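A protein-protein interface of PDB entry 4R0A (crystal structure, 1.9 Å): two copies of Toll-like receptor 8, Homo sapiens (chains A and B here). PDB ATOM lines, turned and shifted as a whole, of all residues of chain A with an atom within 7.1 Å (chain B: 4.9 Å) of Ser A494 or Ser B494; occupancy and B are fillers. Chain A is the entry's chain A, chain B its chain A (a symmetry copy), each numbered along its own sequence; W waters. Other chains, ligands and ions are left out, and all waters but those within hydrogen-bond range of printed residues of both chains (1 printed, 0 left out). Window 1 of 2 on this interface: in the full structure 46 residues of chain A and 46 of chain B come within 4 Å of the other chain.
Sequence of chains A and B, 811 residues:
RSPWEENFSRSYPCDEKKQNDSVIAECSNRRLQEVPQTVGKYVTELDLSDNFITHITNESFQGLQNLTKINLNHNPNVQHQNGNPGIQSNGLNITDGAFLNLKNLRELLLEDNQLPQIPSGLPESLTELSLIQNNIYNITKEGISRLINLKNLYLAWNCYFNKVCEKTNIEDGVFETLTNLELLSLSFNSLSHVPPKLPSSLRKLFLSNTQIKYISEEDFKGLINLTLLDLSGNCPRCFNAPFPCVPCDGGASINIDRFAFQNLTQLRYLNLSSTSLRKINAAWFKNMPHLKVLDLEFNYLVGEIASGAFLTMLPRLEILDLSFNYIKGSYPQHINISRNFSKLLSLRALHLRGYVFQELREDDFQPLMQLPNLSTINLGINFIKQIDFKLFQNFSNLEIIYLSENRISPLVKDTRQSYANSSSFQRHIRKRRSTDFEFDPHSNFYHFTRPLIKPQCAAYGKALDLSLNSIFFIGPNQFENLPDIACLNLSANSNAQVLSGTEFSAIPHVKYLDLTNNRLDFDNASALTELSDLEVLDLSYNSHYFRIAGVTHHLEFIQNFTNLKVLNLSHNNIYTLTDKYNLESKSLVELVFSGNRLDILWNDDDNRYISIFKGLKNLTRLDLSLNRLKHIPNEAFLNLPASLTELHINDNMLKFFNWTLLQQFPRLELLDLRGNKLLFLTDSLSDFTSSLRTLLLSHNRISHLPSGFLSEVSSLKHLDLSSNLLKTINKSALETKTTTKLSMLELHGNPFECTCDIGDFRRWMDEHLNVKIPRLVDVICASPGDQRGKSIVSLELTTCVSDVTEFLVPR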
ATOM      1  N   ASN A 469     -13.511 -18.882  10.576  1.00  0.00           N
ATOM      2  CA  ASN A 469     -12.786 -20.014  10.077  1.00  0.00           C
ATOM      3  C   ASN A 469     -11.635 -19.485   9.209  1.00  0.00           C
ATOM      4  O   ASN A 469     -11.225 -18.316   9.367  1.00  0.00           O
ATOM      5  CB  ASN A 469     -13.706 -20.935   9.296  1.00  0.00           C
ATOM      6  CG  ASN A 469     -14.544 -21.802  10.184  1.00  0.00           C
ATOM      7  OD1 ASN A 469     -14.068 -22.765  10.757  1.00  0.00           O
ATOM      8  ND2 ASN A 469     -15.811 -21.492  10.271  1.00  0.00           N
ATOM      9  N   SER A 470     -11.042 -20.365   8.406  1.00  0.00           N
ATOM     10  CA  SER A 470      -9.910 -19.972   7.566  1.00  0.00           C
ATOM     11  C   SER A 470     -10.178 -20.196   6.081  1.00  0.00           C
ATOM     12  O   SER A 470      -9.304 -20.692   5.347  1.00  0.00           O
ATOM     13  CB  SER A 470      -8.674 -20.738   7.957  1.00  0.00           C
ATOM     14  OG  SER A 470      -8.290 -20.475   9.298  1.00  0.00           O
ATOM     15  N   ILE A 471     -11.375 -19.835   5.628  1.00  0.00           N
ATOM     16  CA  ILE A 471     -11.725 -19.995   4.222  1.00  0.00           C
ATOM     17  C   ILE A 471     -11.197 -18.771   3.494  1.00  0.00           C
ATOM     18  O   ILE A 471     -11.936 -17.821   3.234  1.00  0.00           O
ATOM     19  CB  ILE A 471     -13.246 -20.173   4.023  1.00  0.00           C
ATOM     20  CG1 ILE A 471     -13.782 -21.272   4.972  1.00  0.00           C
ATOM     21  CG2 ILE A 471     -13.592 -20.479   2.550  1.00  0.00           C
ATOM     22  CD1 ILE A 471     -15.297 -21.360   5.036  1.00  0.00           C
ATOM     23  N   PHE A 472      -9.895 -18.770   3.230  1.00  0.00           N
ATOM     24  CA  PHE A 472      -9.192 -17.570   2.806  1.00  0.00           C
ATOM     25  C   PHE A 472      -9.263 -17.293   1.302  1.00  0.00           C
ATOM     26  O   PHE A 472      -8.979 -16.180   0.829  1.00  0.00           O
ATOM     27  CB  PHE A 472      -7.755 -17.546   3.381  1.00  0.00           C
ATOM     28  CG  PHE A 472      -6.787 -18.409   2.665  1.00  0.00           C
ATOM     29  CD1 PHE A 472      -5.971 -17.880   1.665  1.00  0.00           C
ATOM     30  CD2 PHE A 472      -6.678 -19.767   2.972  1.00  0.00           C
ATOM     31  CE1 PHE A 472      -5.077 -18.683   0.989  1.00  0.00           C
ATOM     32  CE2 PHE A 472      -5.761 -20.559   2.305  1.00  0.00           C
ATOM     33  CZ  PHE A 472      -4.961 -20.018   1.321  1.00  0.00           C
ATOM     34  N   PHE A 473      -9.811 -18.254   0.577  1.00  0.00           N
ATOM     35  CA  PHE A 473     -10.373 -18.023  -0.722  1.00  0.00           C
ATOM     36  C   PHE A 473     -11.482 -19.033  -0.945  1.00  0.00           C
ATOM     37  O   PHE A 473     -11.524 -20.053  -0.257  1.00  0.00           O
ATOM     38  CB  PHE A 473      -9.323 -18.163  -1.791  1.00  0.00           C
ATOM     39  CG  PHE A 473      -8.817 -19.558  -1.961  1.00  0.00           C
ATOM     40  CD1 PHE A 473      -9.443 -20.419  -2.855  1.00  0.00           C
ATOM     41  CD2 PHE A 473      -7.708 -19.993  -1.282  1.00  0.00           C
ATOM     42  CE1 PHE A 473      -8.986 -21.714  -3.027  1.00  0.00           C
ATOM     43  CE2 PHE A 473      -7.233 -21.281  -1.461  1.00  0.00           C
ATOM     44  CZ  PHE A 473      -7.879 -22.143  -2.334  1.00  0.00           C
ATOM     45  N   LEU A 490     -19.793 -15.291   6.193  1.00  0.00           N
ATOM     46  CA  LEU A 490     -18.373 -15.601   5.999  1.00  0.00           C
ATOM     47  C   LEU A 490     -17.446 -14.605   6.689  1.00  0.00           C
ATOM     48  O   LEU A 490     -16.313 -14.411   6.235  1.00  0.00           O
ATOM     49  CB  LEU A 490     -18.069 -15.607   4.530  1.00  0.00           C
ATOM     50  CG  LEU A 490     -18.592 -16.823   3.765  1.00  0.00           C
ATOM     51  CD1 LEU A 490     -18.454 -16.573   2.260  1.00  0.00           C
ATOM     52  CD2 LEU A 490     -17.838 -18.073   4.164  1.00  0.00           C
ATOM     53  N   SER A 491     -17.959 -13.911   7.707  1.00  0.00           N
ATOM     54  CA  SER A 491     -17.189 -12.937   8.472  1.00  0.00           C
ATOM     55  C   SER A 491     -15.892 -13.590   9.009  1.00  0.00           C
ATOM     56  O   SER A 491     -15.923 -14.756   9.450  1.00  0.00           O
ATOM     57  CB  SER A 491     -18.010 -12.524   9.687  1.00  0.00           C
ATOM     58  OG  SER A 491     -17.399 -11.452  10.344  1.00  0.00           O
ATOM     59  N   ALA A 492     -14.781 -12.849   9.006  1.00  0.00           N
ATOM     60  CA  ALA A 492     -13.586 -13.241   9.699  1.00  0.00           C
ATOM     61  C   ALA A 492     -13.030 -14.589   9.235  1.00  0.00           C
ATOM     62  O   ALA A 492     -12.643 -15.434  10.049  1.00  0.00           O
ATOM     63  CB  ALA A 492     -13.756 -13.248  11.217  1.00  0.00           C
ATOM     64  N   ASN A 493     -12.958 -14.732   7.932  1.00  0.00           N
ATOM     65  CA  ASN A 493     -12.217 -15.834   7.317  1.00  0.00           C
ATOM     66  C   ASN A 493     -10.876 -15.433   6.681  1.00  0.00           C
ATOM     67  O   ASN A 493     -10.249 -16.223   5.962  1.00  0.00           O
ATOM     68  CB  ASN A 493     -13.128 -16.510   6.285  1.00  0.00           C
ATOM     69  CG  ASN A 493     -13.947 -17.597   6.922  1.00  0.00           C
ATOM     70  OD1 ASN A 493     -13.506 -18.758   6.991  1.00  0.00           O
ATOM     71  ND2 ASN A 493     -15.126 -17.235   7.436  1.00  0.00           N
ATOM     72  N   SER A 494     -10.448 -14.204   6.960  1.00  0.00           N
ATOM     73  CA  SER A 494      -9.272 -13.615   6.313  1.00  0.00           C
ATOM     74  C   SER A 494      -9.248 -13.890   4.838  1.00  0.00           C
ATOM     75  O   SER A 494      -8.195 -14.224   4.245  1.00  0.00           O
ATOM     76  CB  SER A 494      -8.008 -14.138   7.012  1.00  0.00           C
ATOM     77  OG  SER A 494      -8.063 -13.676   8.366  1.00  0.00           O
ATOM     78  N   ASN A 495     -10.405 -13.683   4.218  1.00  0.00           N
ATOM     79  CA  ASN A 495     -10.563 -13.982   2.826  1.00  0.00           C
ATOM     80  C   ASN A 495      -9.990 -12.851   1.966  1.00  0.00           C
ATOM     81  O   ASN A 495     -10.431 -11.700   2.067  1.00  0.00           O
ATOM     82  CB  ASN A 495     -12.044 -14.172   2.484  1.00  0.00           C
ATOM     83  CG  ASN A 495     -12.232 -14.652   1.064  1.00  0.00           C
ATOM     84  OD1 ASN A 495     -11.777 -14.006   0.169  1.00  0.00           O
ATOM     85  ND2 ASN A 495     -12.810 -15.853   0.875  1.00  0.00           N
ATOM     86  N   ALA A 496      -9.072 -13.218   1.077  1.00  0.00           N
ATOM     87  CA  ALA A 496      -8.311 -12.297   0.241  1.00  0.00           C
ATOM     88  C   ALA A 496      -8.706 -12.343  -1.257  1.00  0.00           C
ATOM     89  O   ALA A 496      -8.024 -11.785  -2.110  1.00  0.00           O
ATOM     90  CB  ALA A 496      -6.833 -12.602   0.405  1.00  0.00           C
ATOM     91  N   GLN A 497      -9.859 -12.911  -1.549  1.00  0.00           N
ATOM     92  CA  GLN A 497     -10.261 -13.251  -2.919  1.00  0.00           C
ATOM     93  C   GLN A 497     -10.563 -12.032  -3.731  1.00  0.00           C
ATOM     94  O   GLN A 497     -11.121 -11.045  -3.220  1.00  0.00           O
ATOM     95  CB  GLN A 497     -11.541 -14.080  -2.849  1.00  0.00           C
ATOM     96  CG  GLN A 497     -12.116 -14.516  -4.180  1.00  0.00           C
ATOM     97  CD  GLN A 497     -12.180 -16.014  -4.275  1.00  0.00           C
ATOM     98  OE1 GLN A 497     -12.055 -16.696  -3.270  1.00  0.00           O
ATOM     99  NE2 GLN A 497     -12.309 -16.536  -5.484  1.00  0.00           N
ATOM    100  N   THR A 516     -17.930  -9.375   6.740  1.00  0.00           N
ATOM    101  CA  THR A 516     -17.149  -8.402   7.542  1.00  0.00           C
ATOM    102  C   THR A 516     -15.846  -9.014   8.022  1.00  0.00           C
ATOM    103  O   THR A 516     -15.755 -10.223   8.146  1.00  0.00           O
ATOM    104  CB  THR A 516     -17.899  -7.825   8.755  1.00  0.00           C
ATOM    105  OG1 THR A 516     -17.908  -8.748   9.799  1.00  0.00           O
ATOM    106  CG2 THR A 516     -19.278  -7.495   8.449  1.00  0.00           C
ATOM    107  N   ASN A 517     -14.825  -8.191   8.284  1.00  0.00           N
ATOM    108  CA  ASN A 517     -13.583  -8.667   8.822  1.00  0.00           C
ATOM    109  C   ASN A 517     -12.915  -9.700   7.918  1.00  0.00           C
ATOM    110  O   ASN A 517     -12.494 -10.755   8.366  1.00  0.00           O
ATOM    111  CB  ASN A 517     -13.728  -9.259  10.229  1.00  0.00           C
ATOM    112  CG  ASN A 517     -14.294  -8.272  11.233  1.00  0.00           C
ATOM    113  OD1 ASN A 517     -13.559  -7.617  11.979  1.00  0.00           O
ATOM    114  ND2 ASN A 517     -15.622  -8.200  11.301  1.00  0.00           N
ATOM    115  N   ASN A 518     -12.778  -9.372   6.650  1.00  0.00           N
ATOM    116  CA  ASN A 518     -11.943 -10.191   5.767  1.00  0.00           C
ATOM    117  C   ASN A 518     -10.879  -9.285   5.175  1.00  0.00           C
ATOM    118  O   ASN A 518     -10.683  -8.186   5.697  1.00  0.00           O
ATOM    119  CB  ASN A 518     -12.811 -10.848   4.724  1.00  0.00           C
ATOM    120  CG  ASN A 518     -13.505 -12.078   5.263  1.00  0.00           C
ATOM    121  OD1 ASN A 518     -12.868 -13.116   5.575  1.00  0.00           O
ATOM    122  ND2 ASN A 518     -14.802 -11.985   5.375  1.00  0.00           N
ATOM    123  N   ARG A 519     -10.284  -9.673   4.057  1.00  0.00           N
ATOM    124  CA  ARG A 519      -9.356  -8.794   3.345  1.00  0.00           C
ATOM    125  C   ARG A 519      -9.594  -8.865   1.861  1.00  0.00           C
ATOM    126  O   ARG A 519      -8.691  -9.126   1.072  1.00  0.00           O
ATOM    127  CB  ARG A 519      -7.893  -9.150   3.731  1.00  0.00           C
ATOM    128  CG  ARG A 519      -7.558 -10.620   3.584  1.00  0.00           C
ATOM    129  CD  ARG A 519      -6.071 -10.915   3.763  1.00  0.00           C
ATOM    130  NE  ARG A 519      -5.693 -10.924   5.158  1.00  0.00           N
ATOM    131  CZ  ARG A 519      -4.463 -11.144   5.615  1.00  0.00           C
ATOM    132  NH1 ARG A 519      -3.453 -11.376   4.786  1.00  0.00           N
ATOM    133  NH2 ARG A 519      -4.250 -11.131   6.910  1.00  0.00           N
ATOM    134  N   LEU A 520     -10.822  -8.579   1.444  1.00  0.00           N
ATOM    135  CA  LEU A 520     -11.197  -8.831   0.079  1.00  0.00           C
ATOM    136  C   LEU A 520     -10.457  -7.871  -0.849  1.00  0.00           C
ATOM    137  O   LEU A 520     -10.278  -6.688  -0.538  1.00  0.00           O
ATOM    138  CB  LEU A 520     -12.716  -8.657  -0.126  1.00  0.00           C
ATOM    139  CG  LEU A 520     -13.532  -9.763   0.477  1.00  0.00           C
ATOM    140  CD1 LEU A 520     -14.988  -9.349   0.597  1.00  0.00           C
ATOM    141  CD2 LEU A 520     -13.393 -11.042  -0.373  1.00  0.00           C
ATOM    142  N   ASN B 469       0.402 -11.802   4.685  1.00  0.00           N
ATOM    143  CA  ASN B 469       0.215 -12.898   3.778  1.00  0.00           C
ATOM    144  C   ASN B 469      -0.839 -13.834   4.389  1.00  0.00           C
ATOM    145  O   ASN B 469      -1.635 -13.397   5.245  1.00  0.00           O
ATOM    146  CB  ASN B 469       1.530 -13.613   3.526  1.00  0.00           C
ATOM    147  CG  ASN B 469       2.402 -12.889   2.548  1.00  0.00           C
ATOM    148  OD1 ASN B 469       2.165 -12.910   1.355  1.00  0.00           O
ATOM    149  ND2 ASN B 469       3.447 -12.278   3.042  1.00  0.00           N
ATOM    150  N   PHE B 472      -1.425 -19.326   7.352  1.00  0.00           N
ATOM    151  CA  PHE B 472      -2.381 -19.479   8.438  1.00  0.00           C
ATOM    152  C   PHE B 472      -2.092 -20.656   9.374  1.00  0.00           C
ATOM    153  O   PHE B 472      -2.623 -20.745  10.494  1.00  0.00           O
ATOM    154  CB  PHE B 472      -3.831 -19.448   7.897  1.00  0.00           C
ATOM    155  CG  PHE B 472      -4.285 -20.711   7.271  1.00  0.00           C
ATOM    156  CD1 PHE B 472      -5.002 -21.652   8.012  1.00  0.00           C
ATOM    157  CD2 PHE B 472      -3.998 -20.989   5.933  1.00  0.00           C
ATOM    158  CE1 PHE B 472      -5.415 -22.833   7.435  1.00  0.00           C
ATOM    159  CE2 PHE B 472      -4.440 -22.166   5.357  1.00  0.00           C
ATOM    160  CZ  PHE B 472      -5.148 -23.082   6.104  1.00  0.00           C
ATOM    161  N   ALA B 492      -0.102 -10.492  10.890  1.00  0.00           N
ATOM    162  CA  ALA B 492      -1.217 -10.434   9.986  1.00  0.00           C
ATOM    163  C   ALA B 492      -1.184 -11.523   8.911  1.00  0.00           C
ATOM    164  O   ALA B 492      -1.431 -11.262   7.730  1.00  0.00           O
ATOM    165  CB  ALA B 492      -1.375  -9.065   9.328  1.00  0.00           C
ATOM    166  N   ASN B 493      -0.930 -12.730   9.364  1.00  0.00           N
ATOM    167  CA  ASN B 493      -1.117 -13.919   8.532  1.00  0.00           C
ATOM    168  C   ASN B 493      -2.350 -14.765   8.887  1.00  0.00           C
ATOM    169  O   ASN B 493      -2.514 -15.891   8.396  1.00  0.00           O
ATOM    170  CB  ASN B 493       0.160 -14.764   8.603  1.00  0.00           C
ATOM    171  CG  ASN B 493       1.142 -14.345   7.546  1.00  0.00           C
ATOM    172  OD1 ASN B 493       1.107 -14.865   6.416  1.00  0.00           O
ATOM    173  ND2 ASN B 493       1.999 -13.373   7.873  1.00  0.00           N
ATOM    174  N   SER B 494      -3.210 -14.207   9.736  1.00  0.00           N
ATOM    175  CA  SER B 494      -4.352 -14.938  10.293  1.00  0.00           C
ATOM    176  C   SER B 494      -3.974 -16.327  10.718  1.00  0.00           C
ATOM    177  O   SER B 494      -4.707 -17.315  10.477  1.00  0.00           O
ATOM    178  CB  SER B 494      -5.487 -14.947   9.259  1.00  0.00           C
ATOM    179  OG  SER B 494      -5.874 -13.583   9.057  1.00  0.00           O
ATOM    180  N   ASN B 495      -2.850 -16.403  11.420  1.00  0.00           N
ATOM    181  CA  ASN B 495      -2.314 -17.669  11.825  1.00  0.00           C
ATOM    182  C   ASN B 495      -3.035 -18.183  13.075  1.00  0.00           C
ATOM    183  O   ASN B 495      -3.032 -17.519  14.119  1.00  0.00           O
ATOM    184  CB  ASN B 495      -0.817 -17.545  12.126  1.00  0.00           C
ATOM    185  CG  ASN B 495      -0.187 -18.891  12.392  1.00  0.00           C
ATOM    186  OD1 ASN B 495      -0.633 -19.578  13.262  1.00  0.00           O
ATOM    187  ND2 ASN B 495       0.783 -19.312  11.559  1.00  0.00           N
ATOM    188  N   ALA B 496      -3.572 -19.394  12.968  1.00  0.00           N
ATOM    189  CA  ALA B 496      -4.402 -20.027  13.985  1.00  0.00           C
ATOM    190  C   ALA B 496      -3.711 -21.211  14.707  1.00  0.00           C
ATOM    191  O   ALA B 496      -4.345 -21.968  15.434  1.00  0.00           O
ATOM    192  CB  ALA B 496      -5.695 -20.489  13.337  1.00  0.00           C
ATOM    193  N   ASN B 517      -1.456  -9.366  15.263  1.00  0.00           N
ATOM    194  CA  ASN B 517      -2.553  -9.489  14.346  1.00  0.00           C
ATOM    195  C   ASN B 517      -2.637 -10.880  13.721  1.00  0.00           C
ATOM    196  O   ASN B 517      -2.766 -11.024  12.516  1.00  0.00           O
ATOM    197  CB  ASN B 517      -2.518  -8.442  13.226  1.00  0.00           C
ATOM    198  CG  ASN B 517      -2.534  -7.017  13.745  1.00  0.00           C
ATOM    199  OD1 ASN B 517      -3.584  -6.370  13.821  1.00  0.00           O
ATOM    200  ND2 ASN B 517      -1.351  -6.490  14.055  1.00  0.00           N
ATOM    201  N   ASN B 518      -2.605 -11.902  14.551  1.00  0.00           N
ATOM    202  CA  ASN B 518      -2.918 -13.249  14.067  1.00  0.00           C
ATOM    203  C   ASN B 518      -4.073 -13.777  14.897  1.00  0.00           C
ATOM    204  O   ASN B 518      -4.727 -12.980  15.571  1.00  0.00           O
ATOM    205  CB  ASN B 518      -1.681 -14.109  14.151  1.00  0.00           C
ATOM    206  CG  ASN B 518      -0.748 -13.871  12.987  1.00  0.00           C
ATOM    207  OD1 ASN B 518      -1.055 -14.200  11.813  1.00  0.00           O
ATOM    208  ND2 ASN B 518       0.391 -13.309  13.288  1.00  0.00           N
ATOM    209  N   ARG B 519      -4.258 -15.087  14.943  1.00  0.00           N
ATOM    210  CA  ARG B 519      -5.254 -15.685  15.833  1.00  0.00           C
ATOM    211  C   ARG B 519      -4.700 -16.918  16.493  1.00  0.00           C
ATOM    212  O   ARG B 519      -5.279 -17.998  16.435  1.00  0.00           O
ATOM    213  CB  ARG B 519      -6.562 -15.968  15.043  1.00  0.00           C
ATOM    214  CG  ARG B 519      -6.351 -16.755  13.766  1.00  0.00           C
ATOM    215  CD  ARG B 519      -7.658 -17.203  13.119  1.00  0.00           C
ATOM    216  NE  ARG B 519      -8.295 -16.123  12.399  1.00  0.00           N
ATOM    217  CZ  ARG B 519      -9.449 -16.217  11.744  1.00  0.00           C
ATOM    218  NH1 ARG B 519     -10.129 -17.357  11.707  1.00  0.00           N
ATOM    219  NH2 ARG B 519      -9.921 -15.160  11.124  1.00  0.00           N
HETATM  220  O   HOH W   1      -7.113 -18.118   9.220  1.00  0.00           O
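The guanidinium group of Arg B519 sits at hydrogen-bond distance from the backbone carbonyl oxygen of Ala A492. O of Ala B492 sits at hydrogen-bond distance from NH2 of Arg A519. NH1 of Arg A519 sits at hydrogen-bond distance from O of Asn B469, 2.8 Å away. The side-chain hydroxyl of Ser A494 sits close to the side-chain hydroxyl of Ser B494 (2.3 Å). O of Asn A469 sits at hydrogen-bond distance from NH1 of Arg B519, at 2.8 Å.
N of Ser A494 sits at hydrogen-bond distance from OD1 of Asn A518, at 3.0 Å. The backbone NH of Ser B494 sits at hydrogen-bond distance from the side-chain amide oxygen of Asn B518, 3.0 Å away. The backbone NH (N) of Ala A492 sits at hydrogen-bond distance from the backbone carbonyl oxygen (O) of Thr A516. O of Asn B517 lies close to N of Ala B492, at 3.2 Å. The backbone NH of Arg A519 lies within hydrogen-bond range of the backbone carbonyl oxygen of Asn A495 (2.8 Å). The backbone NH (N) of Arg B519 sits at hydrogen-bond distance from the backbone carbonyl oxygen (O) of Asn B495.
Among the printed residues, merely in contact across the chains: Ser A470 with Phe B472 (3.7 Å), Phe A472 with Phe B472 (3.7 Å), Ser A494 with Arg B519 (3.6 Å) and Arg A519 with Ser B494 (3.6 Å).
Of the printed residues of chain B, Asn A469 touches Arg B519. Ser A494 touches just these residues of chain B: Ser B494 (2.3 Å) and Arg B519 (3.6 Å). Printed residues of chain A within 4 Å of Asn B469: Arg A519 (2.8 Å). Printed residues of chain A within 4 Å of Phe B472: Ser A470 and Phe A472. Ser B494 touches just these residues of chain A: Ser A494 and Arg A519. The nearest printed residue of chain B that does not touch Ser A494 is Asn B493 (5.8 Å). The nearest residue of chain A that does not touch Ser B494 is Ser A470 (4.9 Å). The nearest printed residue of chain B that does not touch Ala A492 is Ser B494 (7.1 Å).
Of the 10 printed residues of chain B, 5 touch a printed residue of chain A. Hydrophobic or aromatic side chains of chain B within 4 Å of the printed part of chain A: Phe B472. Along chain A the printed residues that touch a printed residue of chain B span positions 469 to 519. Among the printed residues, no Asp or Glu carboxylate lies within 4 Å of a Lys or Arg side-chain nitrogen of the other chain.
Asn A469 touches Arg B519, and with the chains exchanged Arg A519 touches Asn B469. Ala A492 touches Arg B519, and with the chains exchanged Arg A519 touches Ala B492. Ser A494 touches its own counterpart, Ser B494. Ser A494 touches Arg B519, and with the chains exchanged Arg A519 touches Ser B494.
Water W1 lies within hydrogen-bond range of the side-chain hydroxyl (OG) of Ser A470 (2.6 Å) and the backbone carbonyl oxygen (O) of Ser B494 (2.8 Å).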
